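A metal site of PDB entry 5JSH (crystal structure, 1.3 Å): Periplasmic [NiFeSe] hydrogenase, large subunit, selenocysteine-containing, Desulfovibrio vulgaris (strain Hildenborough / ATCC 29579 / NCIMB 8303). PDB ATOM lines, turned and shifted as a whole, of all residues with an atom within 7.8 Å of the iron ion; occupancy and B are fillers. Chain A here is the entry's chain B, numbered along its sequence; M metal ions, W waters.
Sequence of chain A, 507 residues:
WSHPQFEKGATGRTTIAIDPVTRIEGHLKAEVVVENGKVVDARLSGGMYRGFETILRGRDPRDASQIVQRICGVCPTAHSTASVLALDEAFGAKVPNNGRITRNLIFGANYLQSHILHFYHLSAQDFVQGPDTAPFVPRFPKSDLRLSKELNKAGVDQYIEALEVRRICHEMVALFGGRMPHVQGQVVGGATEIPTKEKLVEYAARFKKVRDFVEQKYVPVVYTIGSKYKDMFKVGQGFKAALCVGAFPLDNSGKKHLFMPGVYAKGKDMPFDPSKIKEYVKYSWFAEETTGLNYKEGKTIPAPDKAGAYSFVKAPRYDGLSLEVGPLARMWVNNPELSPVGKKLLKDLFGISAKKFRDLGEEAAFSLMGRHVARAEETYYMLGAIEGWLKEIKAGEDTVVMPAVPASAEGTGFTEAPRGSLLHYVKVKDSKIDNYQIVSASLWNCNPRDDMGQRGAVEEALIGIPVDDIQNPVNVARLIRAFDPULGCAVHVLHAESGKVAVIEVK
Three residues have an atom within 4 Å of the iron ion: Glu 53, Ile 438 and His 492.
The iron ion is bound by water W2, water W3, NE2 of His 492, OE2 of Glu 53, O of Ile 438 and water W1.
Water W3 lies within hydrogen-bond range of the side-chain carboxylate of Glu 279 (2.6 Å), the side-chain amide oxygen of Gln 437 (2.7 Å) and the side-chain amino group of Lys 314 (3.0 Å).
Water W1 bridges OE1 of Glu 53 (2.6 Å) and NZ of Lys 314 (3.1 Å).
ND1 of His 492 lies within hydrogen-bond range of O of Cys 489 (2.8 Å).
OE1 of Gln 437 sits close to OE2 of Glu 53 (3.4 Å).
OG1 of Thr 300 is in hydrogen-bond range of OE1 of Glu 53, at 2.7 Å.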
ATOM      1  N   GLU A  53      12.700  -0.237   5.388  1.00  0.00           N
ATOM      2  CA  GLU A  53      12.188  -1.603   5.272  1.00  0.00           C
ATOM      3  C   GLU A  53      13.303  -2.642   5.300  1.00  0.00           C
ATOM      4  O   GLU A  53      13.036  -3.776   5.684  1.00  0.00           O
ATOM      5  CB  GLU A  53      11.339  -1.719   3.994  1.00  0.00           C
ATOM      6  CG  GLU A  53      10.070  -0.868   4.079  1.00  0.00           C
ATOM      7  CD  GLU A  53       9.510  -0.441   2.739  1.00  0.00           C
ATOM      8  OE1 GLU A  53      10.303  -0.290   1.783  1.00  0.00           O
ATOM      9  OE2 GLU A  53       8.284  -0.184   2.683  1.00  0.00           O
ATOM     10  N   GLU A 279       2.320  -2.374  -5.584  1.00  0.00           N
ATOM     11  CA  GLU A 279       3.330  -1.336  -5.762  1.00  0.00           C
ATOM     12  C   GLU A 279       4.185  -1.644  -6.980  1.00  0.00           C
ATOM     13  O   GLU A 279       4.870  -2.680  -7.027  1.00  0.00           O
ATOM     14  CB  GLU A 279       4.187  -1.159  -4.512  1.00  0.00           C
ATOM     15  CG  GLU A 279       3.405  -0.646  -3.330  1.00  0.00           C
ATOM     16  CD  GLU A 279       4.321  -0.250  -2.175  1.00  0.00           C
ATOM     17  OE1 GLU A 279       4.754  -1.150  -1.419  1.00  0.00           O
ATOM     18  OE2 GLU A 279       4.622   0.949  -2.042  1.00  0.00           O
ATOM     19  N   PHE A 286      14.145   0.956  -8.128  1.00  0.00           N
ATOM     20  CA  PHE A 286      14.133  -0.361  -7.487  1.00  0.00           C
ATOM     21  C   PHE A 286      14.241  -1.446  -8.551  1.00  0.00           C
ATOM     22  O   PHE A 286      13.882  -1.232  -9.704  1.00  0.00           O
ATOM     23  CB  PHE A 286      12.865  -0.552  -6.638  1.00  0.00           C
ATOM     24  CG  PHE A 286      12.766   0.450  -5.551  1.00  0.00           C
ATOM     25  CD1 PHE A 286      13.543   0.318  -4.397  1.00  0.00           C
ATOM     26  CD2 PHE A 286      11.982   1.576  -5.698  1.00  0.00           C
ATOM     27  CE1 PHE A 286      13.504   1.287  -3.413  1.00  0.00           C
ATOM     28  CE2 PHE A 286      11.934   2.526  -4.703  1.00  0.00           C
ATOM     29  CZ  PHE A 286      12.704   2.385  -3.568  1.00  0.00           C
ATOM     30  N   TYR A 295       1.746  -5.532  -0.544  1.00  0.00           N
ATOM     31  CA  TYR A 295       2.641  -5.243   0.578  1.00  0.00           C
ATOM     32  C   TYR A 295       2.957  -6.486   1.414  1.00  0.00           C
ATOM     33  O   TYR A 295       4.035  -6.559   2.007  1.00  0.00           O
ATOM     34  CB  TYR A 295       2.083  -4.097   1.443  1.00  0.00           C
ATOM     35  CG  TYR A 295       0.712  -4.414   1.988  1.00  0.00           C
ATOM     36  CD1 TYR A 295       0.565  -5.163   3.140  1.00  0.00           C
ATOM     37  CD2 TYR A 295      -0.438  -4.007   1.317  1.00  0.00           C
ATOM     38  CE1 TYR A 295      -0.695  -5.510   3.610  1.00  0.00           C
ATOM     39  CE2 TYR A 295      -1.679  -4.335   1.772  1.00  0.00           C
ATOM     40  CZ  TYR A 295      -1.817  -5.085   2.921  1.00  0.00           C
ATOM     41  OH  TYR A 295      -3.074  -5.411   3.360  1.00  0.00           O
ATOM     42  N   LYS A 299       8.936  -6.086  -1.405  1.00  0.00           N
ATOM     43  CA  LYS A 299      10.393  -6.175  -1.443  1.00  0.00           C
ATOM     44  C   LYS A 299      10.929  -4.793  -1.750  1.00  0.00           C
ATOM     45  O   LYS A 299      10.324  -4.034  -2.509  1.00  0.00           O
ATOM     46  CB  LYS A 299      10.910  -7.136  -2.511  1.00  0.00           C
ATOM     47  CG  LYS A 299      10.624  -8.597  -2.219  1.00  0.00           C
ATOM     48  CD  LYS A 299      11.295  -9.487  -3.253  1.00  0.00           C
ATOM     49  CE  LYS A 299      11.176 -10.961  -2.885  1.00  0.00           C
ATOM     50  NZ  LYS A 299      11.992 -11.261  -1.681  1.00  0.00           N
ATOM     51  N   THR A 300      12.085  -4.481  -1.171  1.00  0.00           N
ATOM     52  CA  THR A 300      12.697  -3.156  -1.305  1.00  0.00           C
ATOM     53  C   THR A 300      14.168  -3.334  -1.657  1.00  0.00           C
ATOM     54  O   THR A 300      15.014  -3.532  -0.778  1.00  0.00           O
ATOM     55  CB  THR A 300      12.473  -2.329  -0.050  1.00  0.00           C
ATOM     56  OG1 THR A 300      11.072  -2.265   0.189  1.00  0.00           O
ATOM     57  CG2 THR A 300      13.012  -0.912  -0.251  1.00  0.00           C
ATOM     58  N   PHE A 312      12.562   7.700  -6.003  1.00  0.00           N
ATOM     59  CA  PHE A 312      12.644   6.667  -4.970  1.00  0.00           C
ATOM     60  C   PHE A 312      11.286   6.316  -4.368  1.00  0.00           C
ATOM     61  O   PHE A 312      11.205   5.450  -3.484  1.00  0.00           O
ATOM     62  CB  PHE A 312      13.630   7.077  -3.865  1.00  0.00           C
ATOM     63  CG  PHE A 312      15.077   7.036  -4.272  1.00  0.00           C
ATOM     64  CD1 PHE A 312      15.702   5.838  -4.607  1.00  0.00           C
ATOM     65  CD2 PHE A 312      15.841   8.197  -4.296  1.00  0.00           C
ATOM     66  CE1 PHE A 312      17.049   5.797  -4.964  1.00  0.00           C
ATOM     67  CE2 PHE A 312      17.190   8.175  -4.653  1.00  0.00           C
ATOM     68  CZ  PHE A 312      17.801   6.959  -4.995  1.00  0.00           C
ATOM     69  N   LYS A 314       7.876   4.384  -4.731  1.00  0.00           N
ATOM     70  CA  LYS A 314       7.224   3.346  -5.512  1.00  0.00           C
ATOM     71  C   LYS A 314       5.875   3.879  -6.012  1.00  0.00           C
ATOM     72  O   LYS A 314       5.417   4.953  -5.599  1.00  0.00           O
ATOM     73  CB  LYS A 314       6.985   2.087  -4.665  1.00  0.00           C
ATOM     74  CG  LYS A 314       8.246   1.364  -4.185  1.00  0.00           C
ATOM     75  CD  LYS A 314       7.889   0.119  -3.356  1.00  0.00           C
ATOM     76  CE  LYS A 314       9.128  -0.651  -2.894  1.00  0.00           C
ATOM     77  NZ  LYS A 314       8.754  -1.603  -1.797  1.00  0.00           N
ATOM     78  N   LEU A 423      -0.385   2.238   6.043  1.00  0.00           N
ATOM     79  CA  LEU A 423      -0.364   0.891   6.589  1.00  0.00           C
ATOM     80  C   LEU A 423       1.068   0.423   6.779  1.00  0.00           C
ATOM     81  O   LEU A 423       1.980   0.822   6.037  1.00  0.00           O
ATOM     82  CB  LEU A 423      -1.188  -0.104   5.746  1.00  0.00           C
ATOM     83  CG  LEU A 423      -0.582  -0.438   4.400  1.00  0.00           C
ATOM     84  CD1 LEU A 423       0.312  -1.655   4.487  1.00  0.00           C
ATOM     85  CD2 LEU A 423      -1.673  -0.666   3.338  1.00  0.00           C
ATOM     86  N   TYR A 436       9.221  -6.076   6.744  1.00  0.00           N
ATOM     87  CA  TYR A 436       8.433  -4.947   7.225  1.00  0.00           C
ATOM     88  C   TYR A 436       8.187  -4.068   6.007  1.00  0.00           C
ATOM     89  O   TYR A 436       9.155  -3.629   5.368  1.00  0.00           O
ATOM     90  CB  TYR A 436       9.166  -4.195   8.346  1.00  0.00           C
ATOM     91  CG  TYR A 436       8.267  -3.363   9.231  1.00  0.00           C
ATOM     92  CD1 TYR A 436       7.696  -2.168   8.789  1.00  0.00           C
ATOM     93  CD2 TYR A 436       8.015  -3.764  10.545  1.00  0.00           C
ATOM     94  CE1 TYR A 436       6.902  -1.406   9.628  1.00  0.00           C
ATOM     95  CE2 TYR A 436       7.230  -3.013  11.381  1.00  0.00           C
ATOM     96  CZ  TYR A 436       6.660  -1.858  10.925  1.00  0.00           C
ATOM     97  OH  TYR A 436       5.889  -1.140  11.786  1.00  0.00           O
ATOM     98  N   GLN A 437       6.931  -3.825   5.677  1.00  0.00           N
ATOM     99  CA  GLN A 437       6.588  -3.057   4.489  1.00  0.00           C
ATOM    100  C   GLN A 437       5.653  -1.916   4.856  1.00  0.00           C
ATOM    101  O   GLN A 437       4.704  -2.100   5.614  1.00  0.00           O
ATOM    102  CB  GLN A 437       5.976  -3.935   3.397  1.00  0.00           C
ATOM    103  CG  GLN A 437       6.993  -4.831   2.723  1.00  0.00           C
ATOM    104  CD  GLN A 437       7.997  -4.055   1.870  1.00  0.00           C
ATOM    105  OE1 GLN A 437       7.625  -3.142   1.139  1.00  0.00           O
ATOM    106  NE2 GLN A 437       9.251  -4.446   1.928  1.00  0.00           N
ATOM    107  N   ILE A 438       5.950  -0.737   4.310  1.00  0.00           N
ATOM    108  CA  ILE A 438       5.230   0.492   4.632  1.00  0.00           C
ATOM    109  C   ILE A 438       4.630   1.052   3.356  1.00  0.00           C
ATOM    110  O   ILE A 438       5.335   1.205   2.352  1.00  0.00           O
ATOM    111  CB  ILE A 438       6.180   1.500   5.294  1.00  0.00           C
ATOM    112  CG1 ILE A 438       6.613   0.926   6.648  1.00  0.00           C
ATOM    113  CG2 ILE A 438       5.526   2.851   5.440  1.00  0.00           C
ATOM    114  CD1 ILE A 438       7.908   1.428   7.130  1.00  0.00           C
ATOM    115  N   VAL A 439       3.351   1.402   3.406  1.00  0.00           N
ATOM    116  CA  VAL A 439       2.642   2.038   2.302  1.00  0.00           C
ATOM    117  C   VAL A 439       2.020   3.273   2.920  1.00  0.00           C
ATOM    118  O   VAL A 439       1.065   3.169   3.697  1.00  0.00           O
ATOM    119  CB  VAL A 439       1.590   1.099   1.696  1.00  0.00           C
ATOM    120  CG1 VAL A 439       0.848   1.741   0.550  1.00  0.00           C
ATOM    121  CG2 VAL A 439       2.231  -0.216   1.243  1.00  0.00           C
ATOM    122  N   SER A 440       2.597   4.446   2.648  1.00  0.00           N
ATOM    123  CA  SER A 440       2.315   5.677   3.388  1.00  0.00           C
ATOM    124  C   SER A 440       1.493   6.687   2.554  1.00  0.00           C
ATOM    125  O   SER A 440       1.205   6.491   1.360  1.00  0.00           O
ATOM    126  CB  SER A 440       3.631   6.311   3.790  1.00  0.00           C
ATOM    127  OG  SER A 440       4.337   6.662   2.614  1.00  0.00           O
ATOM    128  N   LEU A 443       3.212   8.626  -0.301  1.00  0.00           N
ATOM    129  CA  LEU A 443       3.420   7.620  -1.336  1.00  0.00           C
ATOM    130  C   LEU A 443       2.251   7.588  -2.307  1.00  0.00           C
ATOM    131  O   LEU A 443       2.445   7.558  -3.523  1.00  0.00           O
ATOM    132  CB  LEU A 443       3.629   6.256  -0.678  1.00  0.00           C
ATOM    133  CG  LEU A 443       3.491   5.011  -1.559  1.00  0.00           C
ATOM    134  CD1 LEU A 443       4.662   4.826  -2.535  1.00  0.00           C
ATOM    135  CD2 LEU A 443       3.333   3.821  -0.678  1.00  0.00           C
ATOM    136  N   CYS A 489       8.152  10.391   4.356  1.00  0.00           N
ATOM    137  CA  CYS A 489       7.108   9.363   4.377  1.00  0.00           C
ATOM    138  C   CYS A 489       7.028   8.625   3.050  1.00  0.00           C
ATOM    139  O   CYS A 489       6.893   7.403   3.024  1.00  0.00           O
ATOM    140  CB  CYS A 489       5.765  10.002   4.676  1.00  0.00           C
ATOM    141  SG  CYS A 489       5.523  10.296   6.417  1.00  0.00           S
ATOM    142  N   ALA A 490       7.029   9.359   1.938  1.00  0.00           N
ATOM    143  CA  ALA A 490       6.772   8.731   0.648  1.00  0.00           C
ATOM    144  C   ALA A 490       7.822   7.685   0.318  1.00  0.00           C
ATOM    145  O   ALA A 490       7.493   6.640  -0.253  1.00  0.00           O
ATOM    146  CB  ALA A 490       6.739   9.801  -0.448  1.00  0.00           C
ATOM    147  N   VAL A 491       9.086   7.956   0.635  1.00  0.00           N
ATOM    148  CA  VAL A 491      10.192   7.067   0.259  1.00  0.00           C
ATOM    149  C   VAL A 491      10.549   6.098   1.386  1.00  0.00           C
ATOM    150  O   VAL A 491      10.853   4.935   1.125  1.00  0.00           O
ATOM    151  CB  VAL A 491      11.433   7.887  -0.158  1.00  0.00           C
ATOM    152  CG1 VAL A 491      12.560   6.913  -0.504  1.00  0.00           C
ATOM    153  CG2 VAL A 491      11.117   8.802  -1.342  1.00  0.00           C
ATOM    154  N   HIS A 492      10.669   6.605   2.611  1.00  0.00           N
ATOM    155  CA  HIS A 492      11.155   5.842   3.748  1.00  0.00           C
ATOM    156  C   HIS A 492      12.419   5.033   3.417  1.00  0.00           C
ATOM    157  O   HIS A 492      13.372   5.642   2.847  1.00  0.00           O
ATOM    158  CB  HIS A 492      10.047   4.985   4.416  1.00  0.00           C
ATOM    159  CG  HIS A 492       9.115   4.280   3.459  1.00  0.00           C
ATOM    160  ND1 HIS A 492       8.072   4.904   2.826  1.00  0.00           N
ATOM    161  CD2 HIS A 492       9.064   2.983   3.071  1.00  0.00           C
ATOM    162  CE1 HIS A 492       7.423   4.036   2.069  1.00  0.00           C
ATOM    163  NE2 HIS A 492       8.015   2.863   2.183  1.00  0.00           N
HETATM  164 FE    FE M   1       7.289   1.079   1.168  1.00  0.00          FE
HETATM  165  O   HOH W   1       9.167   1.058  -0.165  1.00  0.00           O
HETATM  166  O   HOH W   2       6.308   2.138  -0.368  1.00  0.00           O
HETATM  167  O   HOH W   3       6.697  -0.797   0.252  1.00  0.00           O
